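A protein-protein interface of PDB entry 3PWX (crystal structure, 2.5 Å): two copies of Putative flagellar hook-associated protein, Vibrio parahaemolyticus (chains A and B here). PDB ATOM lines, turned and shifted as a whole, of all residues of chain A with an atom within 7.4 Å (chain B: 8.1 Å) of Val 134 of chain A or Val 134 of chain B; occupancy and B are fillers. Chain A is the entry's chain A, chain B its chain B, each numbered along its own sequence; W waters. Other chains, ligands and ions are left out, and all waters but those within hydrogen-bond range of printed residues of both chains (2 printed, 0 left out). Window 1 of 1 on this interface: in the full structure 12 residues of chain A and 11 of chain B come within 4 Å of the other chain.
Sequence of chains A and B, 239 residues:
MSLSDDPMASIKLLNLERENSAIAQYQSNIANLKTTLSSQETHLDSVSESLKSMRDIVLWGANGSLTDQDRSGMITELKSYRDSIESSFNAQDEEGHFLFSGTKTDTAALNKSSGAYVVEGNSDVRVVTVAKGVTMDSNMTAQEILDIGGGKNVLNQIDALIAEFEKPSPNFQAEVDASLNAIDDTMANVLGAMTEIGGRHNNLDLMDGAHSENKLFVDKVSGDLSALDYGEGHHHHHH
OH of Tyr 26 of chain A lies close to N of Lys 132 of chain A.
O of Val 128 of chain A sits at hydrogen-bond distance from N of Met 136 of chain A.
O of Asp 137 of chain A is in hydrogen-bond range of NH1 of Arg 200 of chain A, 3.2 Å away.
The backbone NH (N) of Met 136 of chain B is in hydrogen-bond range of the backbone carbonyl oxygen (O) of Val 128 of chain B.
NE of Arg 200 of chain B is in hydrogen-bond range of O of Asp 137 of chain B (2.9 Å).
Hydrophobic or aromatic side chains of chain A within 4 Å of the printed part of chain B: Ala 131, Val 134, Met 136 and Met 207.
Printed residues of chain B that touch a printed residue of chain A: Gly 133, Val 134, Thr 135, Met 136, Asp 137, Arg 200, Asn 203 and Met 207.
Hydrophobic or aromatic side chains of chain B that line the printed part of chain A: Val 134, Met 136 and Met 207.
Along chain B the printed residues that touch a printed residue of chain A span positions 133 to 207.
Among the printed residues, no Asp or Glu carboxylate lies within 4 Å of a Lys or Arg side-chain nitrogen of the other chain.
Of the printed residues of chain B, Ala 131 of chain A touches Asn 203.
Gly 133 of chain A touches just these residues of chain B: Thr 135 (3.8 Å), Met 136 (3.3 Å), Asp 137 (2.9 Å) and Arg 200 (3.7 Å).
Of chain B, only Val 134, Thr 135 and Met 136 come within 4 Å of Val 134 of chain A.
Of the printed residues of chain B, Asp 137 of chain A touches Gly 133.
Printed residues of chain B within 4 Å of Asn 203 of chain A: Met 207 (3.4 Å).
Printed residues of chain B within 4 Å of Met 207 of chain A: Asn 203 (3.7 Å).
Lys 132 of chain B touches none of the printed residues of chain A.
Val 134 of chain B touches just these residues of chain A: Val 134 (3.9 Å), Thr 135 (3.3 Å) and Met 136 (3.5 Å).
His 211 of chain B touches none of the printed residues of chain A.
The nearest residue of chain B that does not touch Val 134 of chain A is Asn 203 of chain B (4.2 Å).
Water W1 lies within hydrogen-bond range of the side-chain hydroxyl (OG1) of Thr 135 of chain A (2.5 Å), the side-chain carboxylate (OD1) of Asp 137 of chain A (2.8 Å), the backbone carbonyl oxygen (O) of Gly 133 of chain B (2.9 Å) and the backbone NH (N) of Thr 135 of chain B (3.5 Å).
Water W2 lies within hydrogen-bond range of the backbone carbonyl oxygen of Lys 132 of chain B (2.6 Å) and the side-chain amide nitrogen of Asn 203 of chain A (2.8 Å).
O of Lys 132 of chain A is in hydrogen-bond range of NH1 of Arg 200 of chain B (3.1 Å).
O of Gly 133 of chain A sits at hydrogen-bond distance from N of Asp 137 of chain B, 2.9 Å away.
O of Thr 135 of chain A is in hydrogen-bond range of N of Thr 135 of chain B (3.0 Å).
The backbone NH of Asp 137 of chain A sits at hydrogen-bond distance from the backbone carbonyl oxygen of Gly 133 of chain B (2.7 Å).
The side-chain amide oxygen (OD1) of Asn 203 of chain A sits close to the side-chain sulfur (SD) of Met 207 of chain B, 3.6 Å away.
The side-chain amide oxygen (OD1) of Asn 203 of chain B lies close to the side-chain sulfur (SD) of Met 207 of chain A, at 3.7 Å.
Gly 133 of chain A touches Thr 135 of chain B, and with the chains exchanged Thr 135 of chain A touches Gly 133 of chain B.
Gly 133 of chain A touches Asp 137 of chain B, and with the chains exchanged Asp 137 of chain A touches Gly 133 of chain B.
Val 134 of chain B touches its own counterpart, Val 134 of chain A.
Thr 135 of chain B touches its own counterpart, Thr 135 of chain A.
Of the 17 pairs that touch across the chains among the printed residues, 14 have their exchanged pair printed and touching as well.
ND2 of Asn 203 of chain B touches CB of Ala 131 of chain A, at 3.7 Å.
Gly 133 of chain A touches Thr 135 of chain B (O to O, 3.8 Å).
CA of Gly 133 of chain A touches NH1 of Arg 200 of chain B, 3.7 Å away.
Val 134 of chain A touches Val 134 of chain B (CG1 to CG1, 3.9 Å).
Val 134 of chain A touches Thr 135 of chain B (CA to O, 3.4 Å).
CG of Met 136 of chain B touches CG2 of Val 134 of chain A, at 3.9 Å.
Gly 133 of chain B touches Thr 135 of chain A (O to O, 3.6 Å).
Val 134 of chain B touches Thr 135 of chain A (CA to O, 3.3 Å).
Gly 133 of chain B touches Met 136 of chain A (O to CA, 3.3 Å).
Met 136 of chain A touches Val 134 of chain B (CE to CG2, 3.5 Å).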
ATOM      1  N   TYR A  26     -14.483  27.289   6.763  1.00  0.00           N
ATOM      2  CA  TYR A  26     -15.190  26.015   6.860  1.00  0.00           C
ATOM      3  C   TYR A  26     -16.676  26.204   6.696  1.00  0.00           C
ATOM      4  O   TYR A  26     -17.319  25.421   6.034  1.00  0.00           O
ATOM      5  CB  TYR A  26     -14.928  25.311   8.164  1.00  0.00           C
ATOM      6  CG  TYR A  26     -13.505  24.843   8.329  1.00  0.00           C
ATOM      7  CD1 TYR A  26     -12.872  24.088   7.344  1.00  0.00           C
ATOM      8  CD2 TYR A  26     -12.799  25.111   9.494  1.00  0.00           C
ATOM      9  CE1 TYR A  26     -11.495  23.629   7.512  1.00  0.00           C
ATOM     10  CE2 TYR A  26     -11.456  24.661   9.661  1.00  0.00           C
ATOM     11  CZ  TYR A  26     -10.818  23.933   8.660  1.00  0.00           C
ATOM     12  OH  TYR A  26      -9.534  23.463   8.861  1.00  0.00           O
ATOM     13  N   VAL A 127     -14.610  14.830  -2.341  1.00  0.00           N
ATOM     14  CA  VAL A 127     -14.720  15.252  -0.951  1.00  0.00           C
ATOM     15  C   VAL A 127     -14.543  16.764  -0.835  1.00  0.00           C
ATOM     16  O   VAL A 127     -13.852  17.431  -1.654  1.00  0.00           O
ATOM     17  CB  VAL A 127     -13.620  14.603  -0.065  1.00  0.00           C
ATOM     18  CG1 VAL A 127     -13.604  13.083  -0.248  1.00  0.00           C
ATOM     19  CG2 VAL A 127     -12.277  15.202  -0.357  1.00  0.00           C
ATOM     20  N   VAL A 128     -15.109  17.267   0.247  1.00  0.00           N
ATOM     21  CA  VAL A 128     -14.980  18.637   0.691  1.00  0.00           C
ATOM     22  C   VAL A 128     -14.615  18.620   2.164  1.00  0.00           C
ATOM     23  O   VAL A 128     -15.227  17.856   2.990  1.00  0.00           O
ATOM     24  CB  VAL A 128     -16.359  19.341   0.470  1.00  0.00           C
ATOM     25  CG1 VAL A 128     -16.608  20.501   1.432  1.00  0.00           C
ATOM     26  CG2 VAL A 128     -16.419  19.813  -0.943  1.00  0.00           C
ATOM     27  N   THR A 129     -13.656  19.475   2.504  1.00  0.00           N
ATOM     28  CA  THR A 129     -13.163  19.653   3.889  1.00  0.00           C
ATOM     29  C   THR A 129     -14.110  20.581   4.640  1.00  0.00           C
ATOM     30  O   THR A 129     -14.392  21.690   4.171  1.00  0.00           O
ATOM     31  CB  THR A 129     -11.792  20.252   3.886  1.00  0.00           C
ATOM     32  OG1 THR A 129     -10.923  19.291   3.293  1.00  0.00           O
ATOM     33  CG2 THR A 129     -11.288  20.533   5.322  1.00  0.00           C
ATOM     34  N   VAL A 130     -14.591  20.150   5.799  1.00  0.00           N
ATOM     35  CA  VAL A 130     -15.649  20.864   6.401  1.00  0.00           C
ATOM     36  C   VAL A 130     -15.313  21.239   7.843  1.00  0.00           C
ATOM     37  O   VAL A 130     -16.126  21.901   8.496  1.00  0.00           O
ATOM     38  CB  VAL A 130     -17.001  20.063   6.300  1.00  0.00           C
ATOM     39  CG1 VAL A 130     -17.377  19.803   4.814  1.00  0.00           C
ATOM     40  CG2 VAL A 130     -16.962  18.751   7.093  1.00  0.00           C
ATOM     41  N   ALA A 131     -14.165  20.757   8.350  1.00  0.00           N
ATOM     42  CA  ALA A 131     -13.552  21.193   9.604  1.00  0.00           C
ATOM     43  C   ALA A 131     -12.156  20.596   9.604  1.00  0.00           C
ATOM     44  O   ALA A 131     -11.893  19.663   8.835  1.00  0.00           O
ATOM     45  CB  ALA A 131     -14.325  20.740  10.855  1.00  0.00           C
ATOM     46  N   LYS A 132     -11.262  21.113  10.458  1.00  0.00           N
ATOM     47  CA  LYS A 132      -9.896  20.672  10.476  1.00  0.00           C
ATOM     48  C   LYS A 132      -9.829  19.170  10.473  1.00  0.00           C
ATOM     49  O   LYS A 132     -10.255  18.538  11.427  1.00  0.00           O
ATOM     50  CB  LYS A 132      -9.174  21.209  11.702  1.00  0.00           C
ATOM     51  CG  LYS A 132      -7.618  21.030  11.608  1.00  0.00           C
ATOM     52  CD  LYS A 132      -7.083  21.498  10.218  1.00  0.00           C
ATOM     53  CE  LYS A 132      -5.569  21.884  10.225  1.00  0.00           C
ATOM     54  NZ  LYS A 132      -4.768  20.812   9.522  1.00  0.00           N
ATOM     55  N   GLY A 133      -9.247  18.611   9.423  1.00  0.00           N
ATOM     56  CA  GLY A 133      -9.108  17.159   9.295  1.00  0.00           C
ATOM     57  C   GLY A 133     -10.392  16.308   9.118  1.00  0.00           C
ATOM     58  O   GLY A 133     -10.376  15.101   9.399  1.00  0.00           O
ATOM     59  N   VAL A 134     -11.476  16.925   8.623  1.00  0.00           N
ATOM     60  CA  VAL A 134     -12.703  16.233   8.421  1.00  0.00           C
ATOM     61  C   VAL A 134     -13.225  16.474   7.003  1.00  0.00           C
ATOM     62  O   VAL A 134     -13.468  17.621   6.626  1.00  0.00           O
ATOM     63  CB  VAL A 134     -13.794  16.713   9.443  1.00  0.00           C
ATOM     64  CG1 VAL A 134     -15.141  15.921   9.235  1.00  0.00           C
ATOM     65  CG2 VAL A 134     -13.253  16.674  10.907  1.00  0.00           C
ATOM     66  N   THR A 135     -13.458  15.409   6.235  1.00  0.00           N
ATOM     67  CA  THR A 135     -14.018  15.597   4.913  1.00  0.00           C
ATOM     68  C   THR A 135     -15.380  14.968   4.786  1.00  0.00           C
ATOM     69  O   THR A 135     -15.706  13.964   5.438  1.00  0.00           O
ATOM     70  CB  THR A 135     -13.144  14.994   3.820  1.00  0.00           C
ATOM     71  OG1 THR A 135     -13.248  13.575   3.922  1.00  0.00           O
ATOM     72  CG2 THR A 135     -11.694  15.441   3.957  1.00  0.00           C
ATOM     73  N   MET A 136     -16.199  15.569   3.951  1.00  0.00           N
ATOM     74  CA  MET A 136     -17.545  15.002   3.733  1.00  0.00           C
ATOM     75  C   MET A 136     -17.653  14.685   2.242  1.00  0.00           C
ATOM     76  O   MET A 136     -17.176  15.494   1.411  1.00  0.00           O
ATOM     77  CB  MET A 136     -18.600  15.994   4.148  1.00  0.00           C
ATOM     78  CG  MET A 136     -19.922  15.794   3.458  1.00  0.00           C
ATOM     79  SD  MET A 136     -20.953  14.404   4.446  1.00  0.00           S
ATOM     80  CE  MET A 136     -20.558  15.294   6.211  1.00  0.00           C
ATOM     81  N   ASP A 137     -18.188  13.514   1.885  1.00  0.00           N
ATOM     82  CA  ASP A 137     -18.338  13.152   0.464  1.00  0.00           C
ATOM     83  C   ASP A 137     -19.430  13.997  -0.131  1.00  0.00           C
ATOM     84  O   ASP A 137     -20.447  14.208   0.488  1.00  0.00           O
ATOM     85  CB  ASP A 137     -18.627  11.653   0.291  1.00  0.00           C
ATOM     86  CG  ASP A 137     -17.478  10.751   0.840  1.00  0.00           C
ATOM     87  OD1 ASP A 137     -16.285  11.207   1.000  1.00  0.00           O
ATOM     88  OD2 ASP A 137     -17.772   9.554   1.101  1.00  0.00           O
ATOM     89  N   GLY A 199     -28.997  12.521   5.220  1.00  0.00           N
ATOM     90  CA  GLY A 199     -28.049  12.251   6.287  1.00  0.00           C
ATOM     91  C   GLY A 199     -26.800  13.124   6.159  1.00  0.00           C
ATOM     92  O   GLY A 199     -26.271  13.615   7.169  1.00  0.00           O
ATOM     93  N   ARG A 200     -26.299  13.332   4.938  1.00  0.00           N
ATOM     94  CA  ARG A 200     -25.206  14.304   4.758  1.00  0.00           C
ATOM     95  C   ARG A 200     -25.562  15.706   5.252  1.00  0.00           C
ATOM     96  O   ARG A 200     -24.890  16.254   6.121  1.00  0.00           O
ATOM     97  CB  ARG A 200     -24.696  14.312   3.330  1.00  0.00           C
ATOM     98  CG  ARG A 200     -23.728  13.118   3.100  1.00  0.00           C
ATOM     99  CD  ARG A 200     -23.298  13.085   1.626  1.00  0.00           C
ATOM    100  NE  ARG A 200     -22.817  11.777   1.226  1.00  0.00           N
ATOM    101  CZ  ARG A 200     -22.517  11.475  -0.030  1.00  0.00           C
ATOM    102  NH1 ARG A 200     -22.656  12.392  -0.994  1.00  0.00           N
ATOM    103  NH2 ARG A 200     -22.077  10.251  -0.332  1.00  0.00           N
ATOM    104  N   ASN A 203     -25.387  15.857   9.070  1.00  0.00           N
ATOM    105  CA  ASN A 203     -24.095  15.798   9.635  1.00  0.00           C
ATOM    106  C   ASN A 203     -23.368  17.143   9.413  1.00  0.00           C
ATOM    107  O   ASN A 203     -22.716  17.685  10.359  1.00  0.00           O
ATOM    108  CB  ASN A 203     -23.392  14.558   9.109  1.00  0.00           C
ATOM    109  CG  ASN A 203     -23.700  13.327   9.959  1.00  0.00           C
ATOM    110  OD1 ASN A 203     -23.875  13.431  11.198  1.00  0.00           O
ATOM    111  ND2 ASN A 203     -23.710  12.170   9.344  1.00  0.00           N
ATOM    112  N   LEU A 204     -23.560  17.741   8.232  1.00  0.00           N
ATOM    113  CA  LEU A 204     -23.066  19.084   7.995  1.00  0.00           C
ATOM    114  C   LEU A 204     -23.596  20.033   9.081  1.00  0.00           C
ATOM    115  O   LEU A 204     -22.838  20.778   9.760  1.00  0.00           O
ATOM    116  CB  LEU A 204     -23.446  19.585   6.617  1.00  0.00           C
ATOM    117  CG  LEU A 204     -22.760  18.865   5.468  1.00  0.00           C
ATOM    118  CD1 LEU A 204     -23.297  19.359   4.169  1.00  0.00           C
ATOM    119  CD2 LEU A 204     -21.231  19.092   5.537  1.00  0.00           C
ATOM    120  N   MET A 207     -21.697  19.843  12.199  1.00  0.00           N
ATOM    121  CA  MET A 207     -20.419  20.564  12.095  1.00  0.00           C
ATOM    122  C   MET A 207     -20.556  22.052  12.118  1.00  0.00           C
ATOM    123  O   MET A 207     -19.766  22.750  12.744  1.00  0.00           O
ATOM    124  CB  MET A 207     -19.750  20.272  10.782  1.00  0.00           C
ATOM    125  CG  MET A 207     -19.470  18.837  10.573  1.00  0.00           C
ATOM    126  SD  MET A 207     -18.005  18.105  11.650  1.00  0.00           S
ATOM    127  CE  MET A 207     -18.096  16.588  10.421  1.00  0.00           C
ATOM    128  N   TYR B  26     -19.578   2.347  13.146  1.00  0.00           N
ATOM    129  CA  TYR B  26     -19.011   3.697  13.134  1.00  0.00           C
ATOM    130  C   TYR B  26     -18.551   4.094  14.474  1.00  0.00           C
ATOM    131  O   TYR B  26     -17.517   4.775  14.581  1.00  0.00           O
ATOM    132  CB  TYR B  26     -19.984   4.758  12.567  1.00  0.00           C
ATOM    133  CG  TYR B  26     -20.314   4.559  11.113  1.00  0.00           C
ATOM    134  CD1 TYR B  26     -19.311   4.511  10.155  1.00  0.00           C
ATOM    135  CD2 TYR B  26     -21.621   4.476  10.675  1.00  0.00           C
ATOM    136  CE1 TYR B  26     -19.593   4.346   8.802  1.00  0.00           C
ATOM    137  CE2 TYR B  26     -21.914   4.296   9.316  1.00  0.00           C
ATOM    138  CZ  TYR B  26     -20.887   4.221   8.410  1.00  0.00           C
ATOM    139  OH  TYR B  26     -21.145   4.059   7.069  1.00  0.00           O
ATOM    140  N   ASN B  29     -15.306   2.424  15.205  1.00  0.00           N
ATOM    141  CA  ASN B  29     -14.278   3.248  14.537  1.00  0.00           C
ATOM    142  C   ASN B  29     -13.990   4.549  15.280  1.00  0.00           C
ATOM    143  O   ASN B  29     -12.837   4.983  15.381  1.00  0.00           O
ATOM    144  CB  ASN B  29     -14.716   3.602  13.113  1.00  0.00           C
ATOM    145  CG  ASN B  29     -14.785   2.391  12.187  1.00  0.00           C
ATOM    146  OD1 ASN B  29     -14.308   1.314  12.506  1.00  0.00           O
ATOM    147  ND2 ASN B  29     -15.392   2.579  11.023  1.00  0.00           N
ATOM    148  N   VAL B 127      -6.723   8.193   7.575  1.00  0.00           N
ATOM    149  CA  VAL B 127      -8.108   8.652   7.719  1.00  0.00           C
ATOM    150  C   VAL B 127      -8.993   7.490   8.259  1.00  0.00           C
ATOM    151  O   VAL B 127      -8.593   6.332   8.235  1.00  0.00           O
ATOM    152  CB  VAL B 127      -8.705   9.172   6.323  1.00  0.00           C
ATOM    153  CG1 VAL B 127      -7.782  10.201   5.610  1.00  0.00           C
ATOM    154  CG2 VAL B 127      -9.037   8.010   5.420  1.00  0.00           C
ATOM    155  N   VAL B 128     -10.216   7.779   8.696  1.00  0.00           N
ATOM    156  CA  VAL B 128     -11.087   6.778   9.329  1.00  0.00           C
ATOM    157  C   VAL B 128     -12.457   7.294   9.064  1.00  0.00           C
ATOM    158  O   VAL B 128     -12.641   8.501   9.119  1.00  0.00           O
ATOM    159  CB  VAL B 128     -10.878   6.740  10.895  1.00  0.00           C
ATOM    160  CG1 VAL B 128     -11.978   5.894  11.627  1.00  0.00           C
ATOM    161  CG2 VAL B 128      -9.446   6.246  11.296  1.00  0.00           C
ATOM    162  N   THR B 129     -13.409   6.393   8.793  1.00  0.00           N
ATOM    163  CA  THR B 129     -14.776   6.717   8.384  1.00  0.00           C
ATOM    164  C   THR B 129     -15.559   6.674   9.669  1.00  0.00           C
ATOM    165  O   THR B 129     -15.676   5.626  10.312  1.00  0.00           O
ATOM    166  CB  THR B 129     -15.313   5.645   7.459  1.00  0.00           C
ATOM    167  OG1 THR B 129     -14.326   5.392   6.467  1.00  0.00           O
ATOM    168  CG2 THR B 129     -16.618   6.060   6.703  1.00  0.00           C
ATOM    169  N   VAL B 130     -16.079   7.820  10.084  1.00  0.00           N
ATOM    170  CA  VAL B 130     -16.759   7.908  11.368  1.00  0.00           C
ATOM    171  C   VAL B 130     -18.234   8.044  11.130  1.00  0.00           C
ATOM    172  O   VAL B 130     -19.026   7.953  12.056  1.00  0.00           O
ATOM    173  CB  VAL B 130     -16.238   9.070  12.206  1.00  0.00           C
ATOM    174  CG1 VAL B 130     -14.721   8.916  12.405  1.00  0.00           C
ATOM    175  CG2 VAL B 130     -16.562  10.359  11.528  1.00  0.00           C
ATOM    176  N   ALA B 131     -18.600   8.257   9.872  1.00  0.00           N
ATOM    177  CA  ALA B 131     -19.984   8.269   9.534  1.00  0.00           C
ATOM    178  C   ALA B 131     -20.064   8.120   8.048  1.00  0.00           C
ATOM    179  O   ALA B 131     -19.067   8.240   7.372  1.00  0.00           O
ATOM    180  CB  ALA B 131     -20.641   9.546  10.000  1.00  0.00           C
ATOM    181  N   LYS B 132     -21.255   7.850   7.539  1.00  0.00           N
ATOM    182  CA  LYS B 132     -21.423   7.614   6.118  1.00  0.00           C
ATOM    183  C   LYS B 132     -20.971   8.886   5.393  1.00  0.00           C
ATOM    184  O   LYS B 132     -21.540   9.963   5.624  1.00  0.00           O
ATOM    185  CB  LYS B 132     -22.882   7.148   5.787  1.00  0.00           C
ATOM    186  CG  LYS B 132     -23.160   6.653   4.325  1.00  0.00           C
ATOM    187  CD  LYS B 132     -21.829   6.281   3.521  1.00  0.00           C
ATOM    188  CE  LYS B 132     -22.072   5.836   2.034  1.00  0.00           C
ATOM    189  NZ  LYS B 132     -20.895   6.117   1.093  1.00  0.00           N
ATOM    190  N   GLY B 133     -19.917   8.756   4.585  1.00  0.00           N
ATOM    191  CA  GLY B 133     -19.458   9.844   3.750  1.00  0.00           C
ATOM    192  C   GLY B 133     -18.533  10.791   4.472  1.00  0.00           C
ATOM    193  O   GLY B 133     -18.008  11.694   3.847  1.00  0.00           O
ATOM    194  N   VAL B 134     -18.247  10.536   5.754  1.00  0.00           N
ATOM    195  CA  VAL B 134     -17.467  11.447   6.598  1.00  0.00           C
ATOM    196  C   VAL B 134     -16.194  10.780   7.039  1.00  0.00           C
ATOM    197  O   VAL B 134     -16.270   9.748   7.709  1.00  0.00           O
ATOM    198  CB  VAL B 134     -18.198  11.780   7.922  1.00  0.00           C
ATOM    199  CG1 VAL B 134     -17.386  12.818   8.757  1.00  0.00           C
ATOM    200  CG2 VAL B 134     -19.545  12.262   7.703  1.00  0.00           C
ATOM    201  N   THR B 135     -15.031  11.367   6.737  1.00  0.00           N
ATOM    202  CA  THR B 135     -13.795  10.734   7.132  1.00  0.00           C
ATOM    203  C   THR B 135     -12.977  11.682   8.003  1.00  0.00           C
ATOM    204  O   THR B 135     -13.036  12.890   7.834  1.00  0.00           O
ATOM    205  CB  THR B 135     -12.950  10.191   5.957  1.00  0.00           C
ATOM    206  OG1 THR B 135     -11.833  11.043   5.710  1.00  0.00           O
ATOM    207  CG2 THR B 135     -13.710   9.965   4.684  1.00  0.00           C
ATOM    208  N   MET B 136     -12.245  11.147   8.967  1.00  0.00           N
ATOM    209  CA  MET B 136     -11.466  12.009   9.808  1.00  0.00           C
ATOM    210  C   MET B 136     -10.011  11.596   9.838  1.00  0.00           C
ATOM    211  O   MET B 136      -9.722  10.406   9.796  1.00  0.00           O
ATOM    212  CB  MET B 136     -12.045  12.047  11.198  1.00  0.00           C
ATOM    213  CG  MET B 136     -13.382  12.775  11.242  1.00  0.00           C
ATOM    214  SD  MET B 136     -13.901  13.335  13.118  1.00  0.00           S
ATOM    215  CE  MET B 136     -15.747  13.954  12.778  1.00  0.00           C
ATOM    216  N   ASP B 137      -9.107  12.576   9.877  1.00  0.00           N
ATOM    217  CA  ASP B 137      -7.637  12.330   9.875  1.00  0.00           C
ATOM    218  C   ASP B 137      -7.184  11.893  11.248  1.00  0.00           C
ATOM    219  O   ASP B 137      -7.505  12.578  12.221  1.00  0.00           O
ATOM    220  CB  ASP B 137      -6.867  13.623   9.682  1.00  0.00           C
ATOM    221  CG  ASP B 137      -7.112  14.283   8.370  1.00  0.00           C
ATOM    222  OD1 ASP B 137      -7.771  13.723   7.459  1.00  0.00           O
ATOM    223  OD2 ASP B 137      -6.529  15.391   8.270  1.00  0.00           O
ATOM    224  N   GLY B 199      -9.616  19.493  19.100  1.00  0.00           N
ATOM    225  CA  GLY B 199     -10.706  19.863  18.201  1.00  0.00           C
ATOM    226  C   GLY B 199     -11.208  18.613  17.479  1.00  0.00           C
ATOM    227  O   GLY B 199     -12.407  18.469  17.161  1.00  0.00           O
ATOM    228  N   ARG B 200     -10.298  17.680  17.229  1.00  0.00           N
ATOM    229  CA  ARG B 200     -10.730  16.402  16.705  1.00  0.00           C
ATOM    230  C   ARG B 200     -11.598  15.592  17.640  1.00  0.00           C
ATOM    231  O   ARG B 200     -12.541  14.975  17.172  1.00  0.00           O
ATOM    232  CB  ARG B 200      -9.557  15.610  16.116  1.00  0.00           C
ATOM    233  CG  ARG B 200      -9.311  16.137  14.725  1.00  0.00           C
ATOM    234  CD  ARG B 200      -8.862  15.099  13.701  1.00  0.00           C
ATOM    235  NE  ARG B 200      -7.413  15.255  13.398  1.00  0.00           N
ATOM    236  CZ  ARG B 200      -6.887  16.379  12.926  1.00  0.00           C
ATOM    237  NH1 ARG B 200      -7.691  17.422  12.746  1.00  0.00           N
ATOM    238  NH2 ARG B 200      -5.571  16.479  12.630  1.00  0.00           N
ATOM    239  N   ASN B 203     -15.015  17.064  17.603  1.00  0.00           N
ATOM    240  CA  ASN B 203     -15.742  16.715  16.377  1.00  0.00           C
ATOM    241  C   ASN B 203     -16.130  15.242  16.343  1.00  0.00           C
ATOM    242  O   ASN B 203     -17.204  14.918  15.879  1.00  0.00           O
ATOM    243  CB  ASN B 203     -14.906  17.102  15.146  1.00  0.00           C
ATOM    244  CG  ASN B 203     -15.166  18.547  14.684  1.00  0.00           C
ATOM    245  OD1 ASN B 203     -16.324  19.086  14.770  1.00  0.00           O
ATOM    246  ND2 ASN B 203     -14.119  19.181  14.176  1.00  0.00           N
ATOM    247  N   LEU B 204     -15.256  14.359  16.848  1.00  0.00           N
ATOM    248  CA  LEU B 204     -15.613  12.952  17.042  1.00  0.00           C
ATOM    249  C   LEU B 204     -16.857  12.867  17.880  1.00  0.00           C
ATOM    250  O   LEU B 204     -17.835  12.303  17.409  1.00  0.00           O
ATOM    251  CB  LEU B 204     -14.498  12.122  17.657  1.00  0.00           C
ATOM    252  CG  LEU B 204     -13.309  11.818  16.731  1.00  0.00           C
ATOM    253  CD1 LEU B 204     -12.199  11.172  17.531  1.00  0.00           C
ATOM    254  CD2 LEU B 204     -13.665  10.908  15.591  1.00  0.00           C
ATOM    255  N   MET B 207     -20.095  13.494  16.320  1.00  0.00           N
ATOM    256  CA  MET B 207     -20.644  12.430  15.457  1.00  0.00           C
ATOM    257  C   MET B 207     -21.066  11.264  16.321  1.00  0.00           C
ATOM    258  O   MET B 207     -22.033  10.601  16.008  1.00  0.00           O
ATOM    259  CB  MET B 207     -19.642  11.944  14.409  1.00  0.00           C
ATOM    260  CG  MET B 207     -19.100  12.979  13.469  1.00  0.00           C
ATOM    261  SD  MET B 207     -20.426  13.324  12.147  1.00  0.00           S
ATOM    262  CE  MET B 207     -21.309  14.827  13.015  1.00  0.00           C
ATOM    263  N   HIS B 211     -24.901   9.400  16.371  1.00  0.00           N
ATOM    264  CA  HIS B 211     -24.981   7.967  16.182  1.00  0.00           C
ATOM    265  C   HIS B 211     -25.775   7.311  17.278  1.00  0.00           C
ATOM    266  O   HIS B 211     -26.469   6.344  17.041  1.00  0.00           O
ATOM    267  CB  HIS B 211     -23.568   7.371  16.176  1.00  0.00           C
ATOM    268  CG  HIS B 211     -22.881   7.450  14.847  1.00  0.00           C
ATOM    269  ND1 HIS B 211     -23.506   7.100  13.665  1.00  0.00           N
ATOM    270  CD2 HIS B 211     -21.617   7.809  14.512  1.00  0.00           C
ATOM    271  CE1 HIS B 211     -22.657   7.252  12.662  1.00  0.00           C
ATOM    272  NE2 HIS B 211     -21.507   7.679  13.144  1.00  0.00           N
HETATM  273  O   HOH W   1     -15.206  12.182   3.389  1.00  0.00           O
HETATM  274  O   HOH W   2     -23.193  11.659   6.615  1.00  0.00           O
